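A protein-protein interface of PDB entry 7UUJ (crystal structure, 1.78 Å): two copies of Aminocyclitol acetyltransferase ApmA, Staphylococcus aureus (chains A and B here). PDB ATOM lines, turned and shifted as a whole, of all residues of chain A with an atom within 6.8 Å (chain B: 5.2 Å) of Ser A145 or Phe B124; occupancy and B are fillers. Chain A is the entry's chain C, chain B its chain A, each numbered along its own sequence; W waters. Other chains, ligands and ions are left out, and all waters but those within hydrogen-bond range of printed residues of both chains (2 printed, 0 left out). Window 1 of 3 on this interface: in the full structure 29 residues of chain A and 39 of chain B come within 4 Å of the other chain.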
ATOM      1  N   HIS A 137      -4.174  30.453 -21.376  1.00  0.00           N
ATOM      2  CA  HIS A 137      -3.526  29.174 -21.680  1.00  0.00           C
ATOM      3  C   HIS A 137      -3.100  28.497 -20.380  1.00  0.00           C
ATOM      4  O   HIS A 137      -3.084  29.115 -19.299  1.00  0.00           O
ATOM      5  CB  HIS A 137      -2.297  29.386 -22.567  1.00  0.00           C
ATOM      6  CG  HIS A 137      -2.626  29.817 -23.968  1.00  0.00           C
ATOM      7  ND1 HIS A 137      -1.775  29.611 -25.032  1.00  0.00           N
ATOM      8  CD2 HIS A 137      -3.733  30.410 -24.483  1.00  0.00           C
ATOM      9  CE1 HIS A 137      -2.326  30.088 -26.139  1.00  0.00           C
ATOM     10  NE2 HIS A 137      -3.518  30.575 -25.835  1.00  0.00           N
ATOM     11  N   GLN A 138      -2.709  27.220 -20.476  1.00  0.00           N
ATOM     12  CA  GLN A 138      -2.182  26.543 -19.290  1.00  0.00           C
ATOM     13  C   GLN A 138      -0.908  27.227 -18.798  1.00  0.00           C
ATOM     14  O   GLN A 138      -0.055  27.638 -19.587  1.00  0.00           O
ATOM     15  CB  GLN A 138      -1.909  25.066 -19.585  1.00  0.00           C
ATOM     16  CG  GLN A 138      -0.692  24.805 -20.473  1.00  0.00           C
ATOM     17  CD  GLN A 138      -0.962  25.052 -21.974  1.00  0.00           C
ATOM     18  OE1 GLN A 138      -2.105  25.250 -22.407  1.00  0.00           O
ATOM     19  NE2 GLN A 138       0.108  25.036 -22.771  1.00  0.00           N
ATOM     20  N   PHE A 143       5.397  24.190 -21.482  1.00  0.00           N
ATOM     21  CA  PHE A 143       5.060  25.098 -22.575  1.00  0.00           C
ATOM     22  C   PHE A 143       3.750  25.813 -22.285  1.00  0.00           C
ATOM     23  O   PHE A 143       2.914  25.333 -21.508  1.00  0.00           O
ATOM     24  CB  PHE A 143       4.915  24.336 -23.911  1.00  0.00           C
ATOM     25  CG  PHE A 143       3.844  23.273 -23.887  1.00  0.00           C
ATOM     26  CD1 PHE A 143       4.110  22.007 -23.361  1.00  0.00           C
ATOM     27  CD2 PHE A 143       2.582  23.532 -24.394  1.00  0.00           C
ATOM     28  CE1 PHE A 143       3.105  21.017 -23.324  1.00  0.00           C
ATOM     29  CE2 PHE A 143       1.577  22.555 -24.381  1.00  0.00           C
ATOM     30  CZ  PHE A 143       1.846  21.295 -23.853  1.00  0.00           C
ATOM     31  N   VAL A 144       3.598  26.991 -22.887  1.00  0.00           N
ATOM     32  CA  VAL A 144       2.371  27.770 -22.776  1.00  0.00           C
ATOM     33  C   VAL A 144       1.564  27.764 -24.077  1.00  0.00           C
ATOM     34  O   VAL A 144       0.362  28.082 -24.055  1.00  0.00           O
ATOM     35  CB  VAL A 144       2.674  29.216 -22.317  1.00  0.00           C
ATOM     36  CG1 VAL A 144       3.405  30.009 -23.430  1.00  0.00           C
ATOM     37  CG2 VAL A 144       1.389  29.944 -21.922  1.00  0.00           C
ATOM     38  N   SER A 145       2.180  27.376 -25.190  1.00  0.00           N
ATOM     39  CA  SER A 145       1.518  27.256 -26.482  1.00  0.00           C
ATOM     40  C   SER A 145       0.267  26.376 -26.444  1.00  0.00           C
ATOM     41  O   SER A 145       0.194  25.356 -25.752  1.00  0.00           O
ATOM     42  CB  SER A 145       2.527  26.689 -27.498  1.00  0.00           C
ATOM     43  OG  SER A 145       1.926  26.349 -28.736  1.00  0.00           O
ATOM     44  N   ASP A 146      -0.734  26.768 -27.241  1.00  0.00           N
ATOM     45  CA  ASP A 146      -1.796  25.819 -27.545  1.00  0.00           C
ATOM     46  C   ASP A 146      -1.571  25.069 -28.861  1.00  0.00           C
ATOM     47  O   ASP A 146      -1.786  23.859 -28.917  1.00  0.00           O
ATOM     48  CB  ASP A 146      -3.159  26.537 -27.570  1.00  0.00           C
ATOM     49  CG  ASP A 146      -3.262  27.616 -28.667  1.00  0.00           C
ATOM     50  OD1 ASP A 146      -2.243  28.273 -29.000  1.00  0.00           O
ATOM     51  OD2 ASP A 146      -4.402  27.841 -29.152  1.00  0.00           O
ATOM     52  N   ASP A 147      -1.127  25.726 -29.933  1.00  0.00           N
ATOM     53  CA  ASP A 147      -1.104  25.070 -31.239  1.00  0.00           C
ATOM     54  C   ASP A 147       0.038  24.042 -31.396  1.00  0.00           C
ATOM     55  O   ASP A 147       0.079  23.335 -32.412  1.00  0.00           O
ATOM     56  CB  ASP A 147      -1.066  26.134 -32.328  1.00  0.00           C
ATOM     57  CG  ASP A 147      -2.468  26.640 -32.684  1.00  0.00           C
ATOM     58  OD1 ASP A 147      -3.439  26.057 -32.149  1.00  0.00           O
ATOM     59  OD2 ASP A 147      -2.620  27.626 -33.455  1.00  0.00           O
ATOM     60  N   ILE A 148       0.930  23.919 -30.409  1.00  0.00           N
ATOM     61  CA  ILE A 148       1.801  22.733 -30.340  1.00  0.00           C
ATOM     62  C   ILE A 148       0.960  21.462 -30.418  1.00  0.00           C
ATOM     63  O   ILE A 148       1.416  20.442 -30.928  1.00  0.00           O
ATOM     64  CB  ILE A 148       2.654  22.793 -29.059  1.00  0.00           C
ATOM     65  CG1 ILE A 148       3.737  21.712 -29.053  1.00  0.00           C
ATOM     66  CG2 ILE A 148       1.777  22.633 -27.798  1.00  0.00           C
ATOM     67  CD1 ILE A 148       4.504  21.640 -27.730  1.00  0.00           C
ATOM     68  N   GLN A 149      -0.294  21.507 -29.947  1.00  0.00           N
ATOM     69  CA  GLN A 149      -1.111  20.294 -29.958  1.00  0.00           C
ATOM     70  C   GLN A 149      -1.431  19.839 -31.376  1.00  0.00           C
ATOM     71  O   GLN A 149      -1.819  18.680 -31.581  1.00  0.00           O
ATOM     72  CB  GLN A 149      -2.399  20.534 -29.154  1.00  0.00           C
ATOM     73  CG  GLN A 149      -3.508  21.236 -29.930  1.00  0.00           C
ATOM     74  CD  GLN A 149      -4.686  21.679 -29.038  1.00  0.00           C
ATOM     75  OE1 GLN A 149      -5.238  22.763 -29.221  1.00  0.00           O
ATOM     76  NE2 GLN A 149      -5.074  20.832 -28.094  1.00  0.00           N
ATOM     77  N   PHE A 151       0.621  19.128 -33.366  1.00  0.00           N
ATOM     78  CA  PHE A 151       1.670  18.137 -33.575  1.00  0.00           C
ATOM     79  C   PHE A 151       1.525  16.911 -32.675  1.00  0.00           C
ATOM     80  O   PHE A 151       2.353  16.001 -32.777  1.00  0.00           O
ATOM     81  CB  PHE A 151       3.053  18.777 -33.342  1.00  0.00           C
ATOM     82  CG  PHE A 151       3.521  19.691 -34.464  1.00  0.00           C
ATOM     83  CD1 PHE A 151       3.051  19.547 -35.764  1.00  0.00           C
ATOM     84  CD2 PHE A 151       4.480  20.686 -34.198  1.00  0.00           C
ATOM     85  CE1 PHE A 151       3.512  20.382 -36.798  1.00  0.00           C
ATOM     86  CE2 PHE A 151       4.947  21.493 -35.209  1.00  0.00           C
ATOM     87  CZ  PHE A 151       4.466  21.353 -36.512  1.00  0.00           C
ATOM     88  N   PHE A 160      -2.253  15.541 -22.660  1.00  0.00           N
ATOM     89  CA  PHE A 160      -2.403  16.994 -22.607  1.00  0.00           C
ATOM     90  C   PHE A 160      -3.798  17.390 -22.143  1.00  0.00           C
ATOM     91  O   PHE A 160      -3.961  18.161 -21.188  1.00  0.00           O
ATOM     92  CB  PHE A 160      -2.107  17.553 -24.002  1.00  0.00           C
ATOM     93  CG  PHE A 160      -2.279  19.047 -24.138  1.00  0.00           C
ATOM     94  CD1 PHE A 160      -1.628  19.924 -23.265  1.00  0.00           C
ATOM     95  CD2 PHE A 160      -3.052  19.571 -25.172  1.00  0.00           C
ATOM     96  CE1 PHE A 160      -1.747  21.275 -23.393  1.00  0.00           C
ATOM     97  CE2 PHE A 160      -3.197  20.943 -25.315  1.00  0.00           C
ATOM     98  CZ  PHE A 160      -2.526  21.813 -24.426  1.00  0.00           C
ATOM     99  N   TYR A 172      -8.231  27.667 -20.930  1.00  0.00           N
ATOM    100  CA  TYR A 172      -9.194  27.566 -22.027  1.00  0.00           C
ATOM    101  C   TYR A 172     -10.626  27.476 -21.515  1.00  0.00           C
ATOM    102  O   TYR A 172     -11.493  26.961 -22.206  1.00  0.00           O
ATOM    103  CB  TYR A 172      -8.864  26.388 -22.953  1.00  0.00           C
ATOM    104  CG  TYR A 172      -7.389  26.379 -23.340  1.00  0.00           C
ATOM    105  CD1 TYR A 172      -6.890  27.328 -24.258  1.00  0.00           C
ATOM    106  CD2 TYR A 172      -6.496  25.468 -22.769  1.00  0.00           C
ATOM    107  CE1 TYR A 172      -5.556  27.373 -24.601  1.00  0.00           C
ATOM    108  CE2 TYR A 172      -5.133  25.492 -23.103  1.00  0.00           C
ATOM    109  CZ  TYR A 172      -4.674  26.449 -24.014  1.00  0.00           C
ATOM    110  OH  TYR A 172      -3.339  26.495 -24.337  1.00  0.00           O
ATOM    111  N   GLY B 100       8.081  31.037 -36.812  1.00  0.00           N
ATOM    112  CA  GLY B 100       8.247  29.627 -36.510  1.00  0.00           C
ATOM    113  C   GLY B 100       6.962  28.839 -36.686  1.00  0.00           C
ATOM    114  O   GLY B 100       5.914  29.361 -37.056  1.00  0.00           O
ATOM    115  N   ARG B 101       7.059  27.525 -36.440  1.00  0.00           N
ATOM    116  CA  ARG B 101       5.921  26.636 -36.589  1.00  0.00           C
ATOM    117  C   ARG B 101       4.894  26.899 -35.514  1.00  0.00           C
ATOM    118  O   ARG B 101       5.248  27.178 -34.361  1.00  0.00           O
ATOM    119  CB  ARG B 101       6.380  25.171 -36.460  1.00  0.00           C
ATOM    120  CG  ARG B 101       7.437  24.761 -37.479  1.00  0.00           C
ATOM    121  CD  ARG B 101       8.052  23.379 -37.103  1.00  0.00           C
ATOM    122  NE  ARG B 101       8.816  23.482 -35.859  1.00  0.00           N
ATOM    123  CZ  ARG B 101       9.229  22.436 -35.145  1.00  0.00           C
ATOM    124  NH1 ARG B 101       8.988  21.194 -35.536  1.00  0.00           N
ATOM    125  NH2 ARG B 101       9.919  22.640 -34.021  1.00  0.00           N
ATOM    126  N   GLN B 102       3.619  26.752 -35.894  1.00  0.00           N
ATOM    127  CA  GLN B 102       2.480  26.817 -34.975  1.00  0.00           C
ATOM    128  C   GLN B 102       2.504  28.129 -34.189  1.00  0.00           C
ATOM    129  O   GLN B 102       2.213  28.165 -32.987  1.00  0.00           O
ATOM    130  CB  GLN B 102       2.428  25.599 -34.031  1.00  0.00           C
ATOM    131  CG  GLN B 102       2.462  24.214 -34.757  1.00  0.00           C
ATOM    132  CD  GLN B 102       1.212  23.935 -35.591  1.00  0.00           C
ATOM    133  OE1 GLN B 102       0.238  24.710 -35.567  1.00  0.00           O
ATOM    134  NE2 GLN B 102       1.224  22.805 -36.341  1.00  0.00           N
ATOM    135  N   THR B 103       2.850  29.215 -34.902  1.00  0.00           N
ATOM    136  CA  THR B 103       2.932  30.554 -34.364  1.00  0.00           C
ATOM    137  C   THR B 103       1.891  31.408 -35.068  1.00  0.00           C
ATOM    138  O   THR B 103       1.779  31.363 -36.304  1.00  0.00           O
ATOM    139  CB  THR B 103       4.350  31.122 -34.511  1.00  0.00           C
ATOM    140  OG1 THR B 103       5.189  30.456 -33.550  1.00  0.00           O
ATOM    141  CG2 THR B 103       4.389  32.654 -34.236  1.00  0.00           C
ATOM    142  N   GLY B 122       9.419  33.485 -32.977  1.00  0.00           N
ATOM    143  CA  GLY B 122       9.823  32.121 -32.715  1.00  0.00           C
ATOM    144  C   GLY B 122       8.735  31.084 -32.983  1.00  0.00           C
ATOM    145  O   GLY B 122       7.669  31.358 -33.543  1.00  0.00           O
ATOM    146  N   GLN B 123       9.027  29.854 -32.522  1.00  0.00           N
ATOM    147  CA  GLN B 123       8.168  28.687 -32.682  1.00  0.00           C
ATOM    148  C   GLN B 123       7.177  28.577 -31.524  1.00  0.00           C
ATOM    149  O   GLN B 123       7.491  28.933 -30.374  1.00  0.00           O
ATOM    150  CB  GLN B 123       9.027  27.400 -32.728  1.00  0.00           C
ATOM    151  CG  GLN B 123      10.318  27.520 -33.543  1.00  0.00           C
ATOM    152  CD  GLN B 123      10.376  26.475 -34.627  1.00  0.00           C
ATOM    153  OE1 GLN B 123       9.371  26.258 -35.326  1.00  0.00           O
ATOM    154  NE2 GLN B 123      11.551  25.795 -34.775  1.00  0.00           N
ATOM    155  N   PHE B 124       5.963  28.113 -31.838  1.00  0.00           N
ATOM    156  CA  PHE B 124       4.928  27.837 -30.822  1.00  0.00           C
ATOM    157  C   PHE B 124       4.612  29.083 -30.008  1.00  0.00           C
ATOM    158  O   PHE B 124       4.431  29.032 -28.791  1.00  0.00           O
ATOM    159  CB  PHE B 124       5.343  26.665 -29.912  1.00  0.00           C
ATOM    160  CG  PHE B 124       5.710  25.444 -30.686  1.00  0.00           C
ATOM    161  CD1 PHE B 124       4.721  24.701 -31.336  1.00  0.00           C
ATOM    162  CD2 PHE B 124       7.055  25.059 -30.814  1.00  0.00           C
ATOM    163  CE1 PHE B 124       5.026  23.571 -32.105  1.00  0.00           C
ATOM    164  CE2 PHE B 124       7.373  23.906 -31.578  1.00  0.00           C
ATOM    165  CZ  PHE B 124       6.358  23.168 -32.216  1.00  0.00           C
ATOM    166  N   THR B 125       4.474  30.207 -30.703  1.00  0.00           N
ATOM    167  CA  THR B 125       4.231  31.476 -30.048  1.00  0.00           C
ATOM    168  C   THR B 125       2.828  31.941 -30.376  1.00  0.00           C
ATOM    169  O   THR B 125       2.378  31.786 -31.515  1.00  0.00           O
ATOM    170  CB  THR B 125       5.303  32.481 -30.457  1.00  0.00           C
ATOM    171  OG1 THR B 125       6.476  32.219 -29.671  1.00  0.00           O
ATOM    172  CG2 THR B 125       4.807  33.947 -30.298  1.00  0.00           C
ATOM    173  N   SER B 126       2.116  32.426 -29.352  1.00  0.00           N
ATOM    174  CA  SER B 126       0.673  32.680 -29.409  1.00  0.00           C
ATOM    175  C   SER B 126       0.439  34.153 -29.121  1.00  0.00           C
ATOM    176  O   SER B 126       0.596  34.595 -27.978  1.00  0.00           O
ATOM    177  CB  SER B 126      -0.071  31.828 -28.377  1.00  0.00           C
ATOM    178  OG  SER B 126       0.312  30.461 -28.466  1.00  0.00           O
ATOM    179  N   SER B 183      10.343  32.071 -28.750  1.00  0.00           N
ATOM    180  CA  SER B 183       9.501  30.883 -28.875  1.00  0.00           C
ATOM    181  C   SER B 183       8.770  30.633 -27.561  1.00  0.00           C
ATOM    182  O   SER B 183       9.226  31.069 -26.486  1.00  0.00           O
ATOM    183  CB  SER B 183      10.355  29.643 -29.238  1.00  0.00           C
ATOM    184  OG  SER B 183      11.072  29.777 -30.472  1.00  0.00           O
ATOM    185  N   ASP B 184       7.634  29.918 -27.667  1.00  0.00           N
ATOM    186  CA  ASP B 184       6.779  29.608 -26.509  1.00  0.00           C
ATOM    187  C   ASP B 184       6.390  30.887 -25.784  1.00  0.00           C
ATOM    188  O   ASP B 184       6.317  30.947 -24.550  1.00  0.00           O
ATOM    189  CB  ASP B 184       7.456  28.585 -25.565  1.00  0.00           C
ATOM    190  CG  ASP B 184       6.495  28.025 -24.516  1.00  0.00           C
ATOM    191  OD1 ASP B 184       5.332  27.735 -24.901  1.00  0.00           O
ATOM    192  OD2 ASP B 184       6.891  27.927 -23.328  1.00  0.00           O
ATOM    193  N   VAL B 185       6.127  31.943 -26.568  1.00  0.00           N
ATOM    194  CA  VAL B 185       5.740  33.240 -26.018  1.00  0.00           C
ATOM    195  C   VAL B 185       4.218  33.325 -26.057  1.00  0.00           C
ATOM    196  O   VAL B 185       3.584  32.819 -26.996  1.00  0.00           O
ATOM    197  CB  VAL B 185       6.397  34.379 -26.828  1.00  0.00           C
ATOM    198  CG1 VAL B 185       5.714  35.744 -26.544  1.00  0.00           C
ATOM    199  CG2 VAL B 185       7.897  34.438 -26.504  1.00  0.00           C
ATOM    200  N   TRP B 248      13.464  22.947 -26.824  1.00  0.00           N
ATOM    201  CA  TRP B 248      12.440  21.980 -27.232  1.00  0.00           C
ATOM    202  C   TRP B 248      11.596  22.530 -28.378  1.00  0.00           C
ATOM    203  O   TRP B 248      11.040  21.752 -29.183  1.00  0.00           O
ATOM    204  CB  TRP B 248      11.539  21.582 -26.027  1.00  0.00           C
ATOM    205  CG  TRP B 248      10.590  22.693 -25.529  1.00  0.00           C
ATOM    206  CD1 TRP B 248      10.749  23.475 -24.381  1.00  0.00           C
ATOM    207  CD2 TRP B 248       9.391  23.161 -26.166  1.00  0.00           C
ATOM    208  NE1 TRP B 248       9.715  24.380 -24.293  1.00  0.00           N
ATOM    209  CE2 TRP B 248       8.878  24.225 -25.374  1.00  0.00           C
ATOM    210  CE3 TRP B 248       8.711  22.801 -27.335  1.00  0.00           C
ATOM    211  CZ2 TRP B 248       7.718  24.901 -25.702  1.00  0.00           C
ATOM    212  CZ3 TRP B 248       7.544  23.508 -27.679  1.00  0.00           C
ATOM    213  CH2 TRP B 248       7.060  24.538 -26.855  1.00  0.00           C
ATOM    214  N   TRP B 249      11.468  23.877 -28.464  1.00  0.00           N
ATOM    215  CA  TRP B 249      10.725  24.501 -29.553  1.00  0.00           C
ATOM    216  C   TRP B 249      11.375  24.274 -30.917  1.00  0.00           C
ATOM    217  O   TRP B 249      10.725  24.531 -31.942  1.00  0.00           O
ATOM    218  CB  TRP B 249      10.569  26.013 -29.279  1.00  0.00           C
ATOM    219  CG  TRP B 249      11.785  26.676 -28.721  1.00  0.00           C
ATOM    220  CD1 TRP B 249      12.867  27.084 -29.423  1.00  0.00           C
ATOM    221  CD2 TRP B 249      12.047  27.017 -27.337  1.00  0.00           C
ATOM    222  NE1 TRP B 249      13.789  27.690 -28.568  1.00  0.00           N
ATOM    223  CE2 TRP B 249      13.295  27.669 -27.295  1.00  0.00           C
ATOM    224  CE3 TRP B 249      11.324  26.863 -26.147  1.00  0.00           C
ATOM    225  CZ2 TRP B 249      13.869  28.139 -26.100  1.00  0.00           C
ATOM    226  CZ3 TRP B 249      11.879  27.352 -24.948  1.00  0.00           C
ATOM    227  CH2 TRP B 249      13.147  27.970 -24.941  1.00  0.00           C
ATOM    228  N   ILE B 256       8.830  15.788 -30.268  1.00  0.00           N
ATOM    229  CA  ILE B 256       7.775  16.350 -29.424  1.00  0.00           C
ATOM    230  C   ILE B 256       6.897  15.229 -28.862  1.00  0.00           C
ATOM    231  O   ILE B 256       6.540  15.227 -27.678  1.00  0.00           O
ATOM    232  CB  ILE B 256       6.938  17.369 -30.240  1.00  0.00           C
ATOM    233  CG1 ILE B 256       7.762  18.629 -30.516  1.00  0.00           C
ATOM    234  CG2 ILE B 256       5.625  17.671 -29.517  1.00  0.00           C
ATOM    235  CD1 ILE B 256       7.057  19.659 -31.483  1.00  0.00           C
HETATM  236  O   HOH W   1       2.674  30.181 -26.976  1.00  0.00           O
HETATM  237  O   HOH W   2       1.089  28.357 -30.353  1.00  0.00           O
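N of Asp B184 is in hydrogen-bond range of O of Gln B123. The side-chain hydroxyl (OG1) of Thr B125 lies within hydrogen-bond range of the backbone NH (N) of Asp B184 (3.3 Å). The backbone carbonyl oxygen (O) of Val B185 is in hydrogen-bond range of the backbone NH (N) of Ser B126. The side-chain amide nitrogen (NE2) of Gln A138 sits at hydrogen-bond distance from the backbone carbonyl oxygen (O) of Phe A143 (3.1 Å). The side-chain amide nitrogen (NE2) of Gln A138 sits at hydrogen-bond distance from the backbone carbonyl oxygen (O) of Ser A145 (3.0 Å). The backbone NH (N) of Asp A147 sits at hydrogen-bond distance from the side-chain hydroxyl (OG) of Ser A145, 3.3 Å away.
Water W2 lies within hydrogen-bond range of OG of Ser A145, O of Gln B102, OG of Ser B126 and N of Asp A147. Water W1 lies within hydrogen-bond range of O of Phe B124 (2.8 Å), O of Val B185 (2.8 Å), OG of Ser B126 (2.8 Å) and N of Ser A145 (3.4 Å).
Among the printed residues, pairs that only touch across the chains: Ser A145 with Phe B124, Phe A151 with Gln B102, Phe A143 with Trp B248, Phe A143 with Asp B184, His A137 with Ser B126, Ile A148 with Trp B248, Phe A151 with Phe B124, Ile A148 with Phe B124, Phe A151 with Ile B256 and Ser A145 with Ser B126.
Of the printed residues of chain B, Ser A145 touches Phe B124 (3.3 Å), Ser B126 (3.96 Å) and Asp B184 (3.2 Å). Phe B124 touches just these residues of chain A: Ser A145 (3.3 Å), Ile A148 (3.6 Å) and Phe A151 (3.6 Å). Printed residues of chain A within 4 Å of Trp B248: Phe A143 and Ile A148. Printed residues of chain A within 4 Å of Gln B102: Asp A147 (3.4 Å) and Phe A151 (3.4 Å). Gln A138 touches none of the printed residues of chain B. The nearest residue of chain B that does not touch Ser A145 is Gln B102 (4.6 Å). The nearest residue of chain A that does not touch Phe B124 is Asp A147 (4.7 Å).
The side-chain amide oxygen (OE1) of Gln B102 sits close to the backbone carbonyl oxygen (O) of Asp A147. The side-chain carboxylate (OD1) of Asp A146 is in hydrogen-bond range of the side-chain hydroxyl (OG) of Ser B126 (3.4 Å). The backbone NH (N) of Val A144 lies within hydrogen-bond range of the side-chain carboxylate (OD1) of Asp B184 (2.8 Å). The side-chain carboxylate (OD1) of Asp B184 sits at hydrogen-bond distance from the backbone NH (N) of Ser A145, 3.2 Å away.
No position is printed for both chains. Of the 14 pairs that touch across the chains among the printed residues, none has its exchanged pair printed and touching as well.
Of the 15 printed residues of chain B, 6 touch a printed residue of chain A. Hydrophobic or aromatic side chains of chain B within 4 Å of the printed part of chain A: Phe B124, Trp B248 and Ile B256. Of the 12 printed residues of chain A, 8 touch a printed residue of chain B. Along chain A the printed residues that touch a printed residue of chain B span positions 137 to 151. Among the printed residues, no Asp or Glu carboxylate lies within 4 Å of a Lys or Arg side-chain nitrogen of the other chain.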
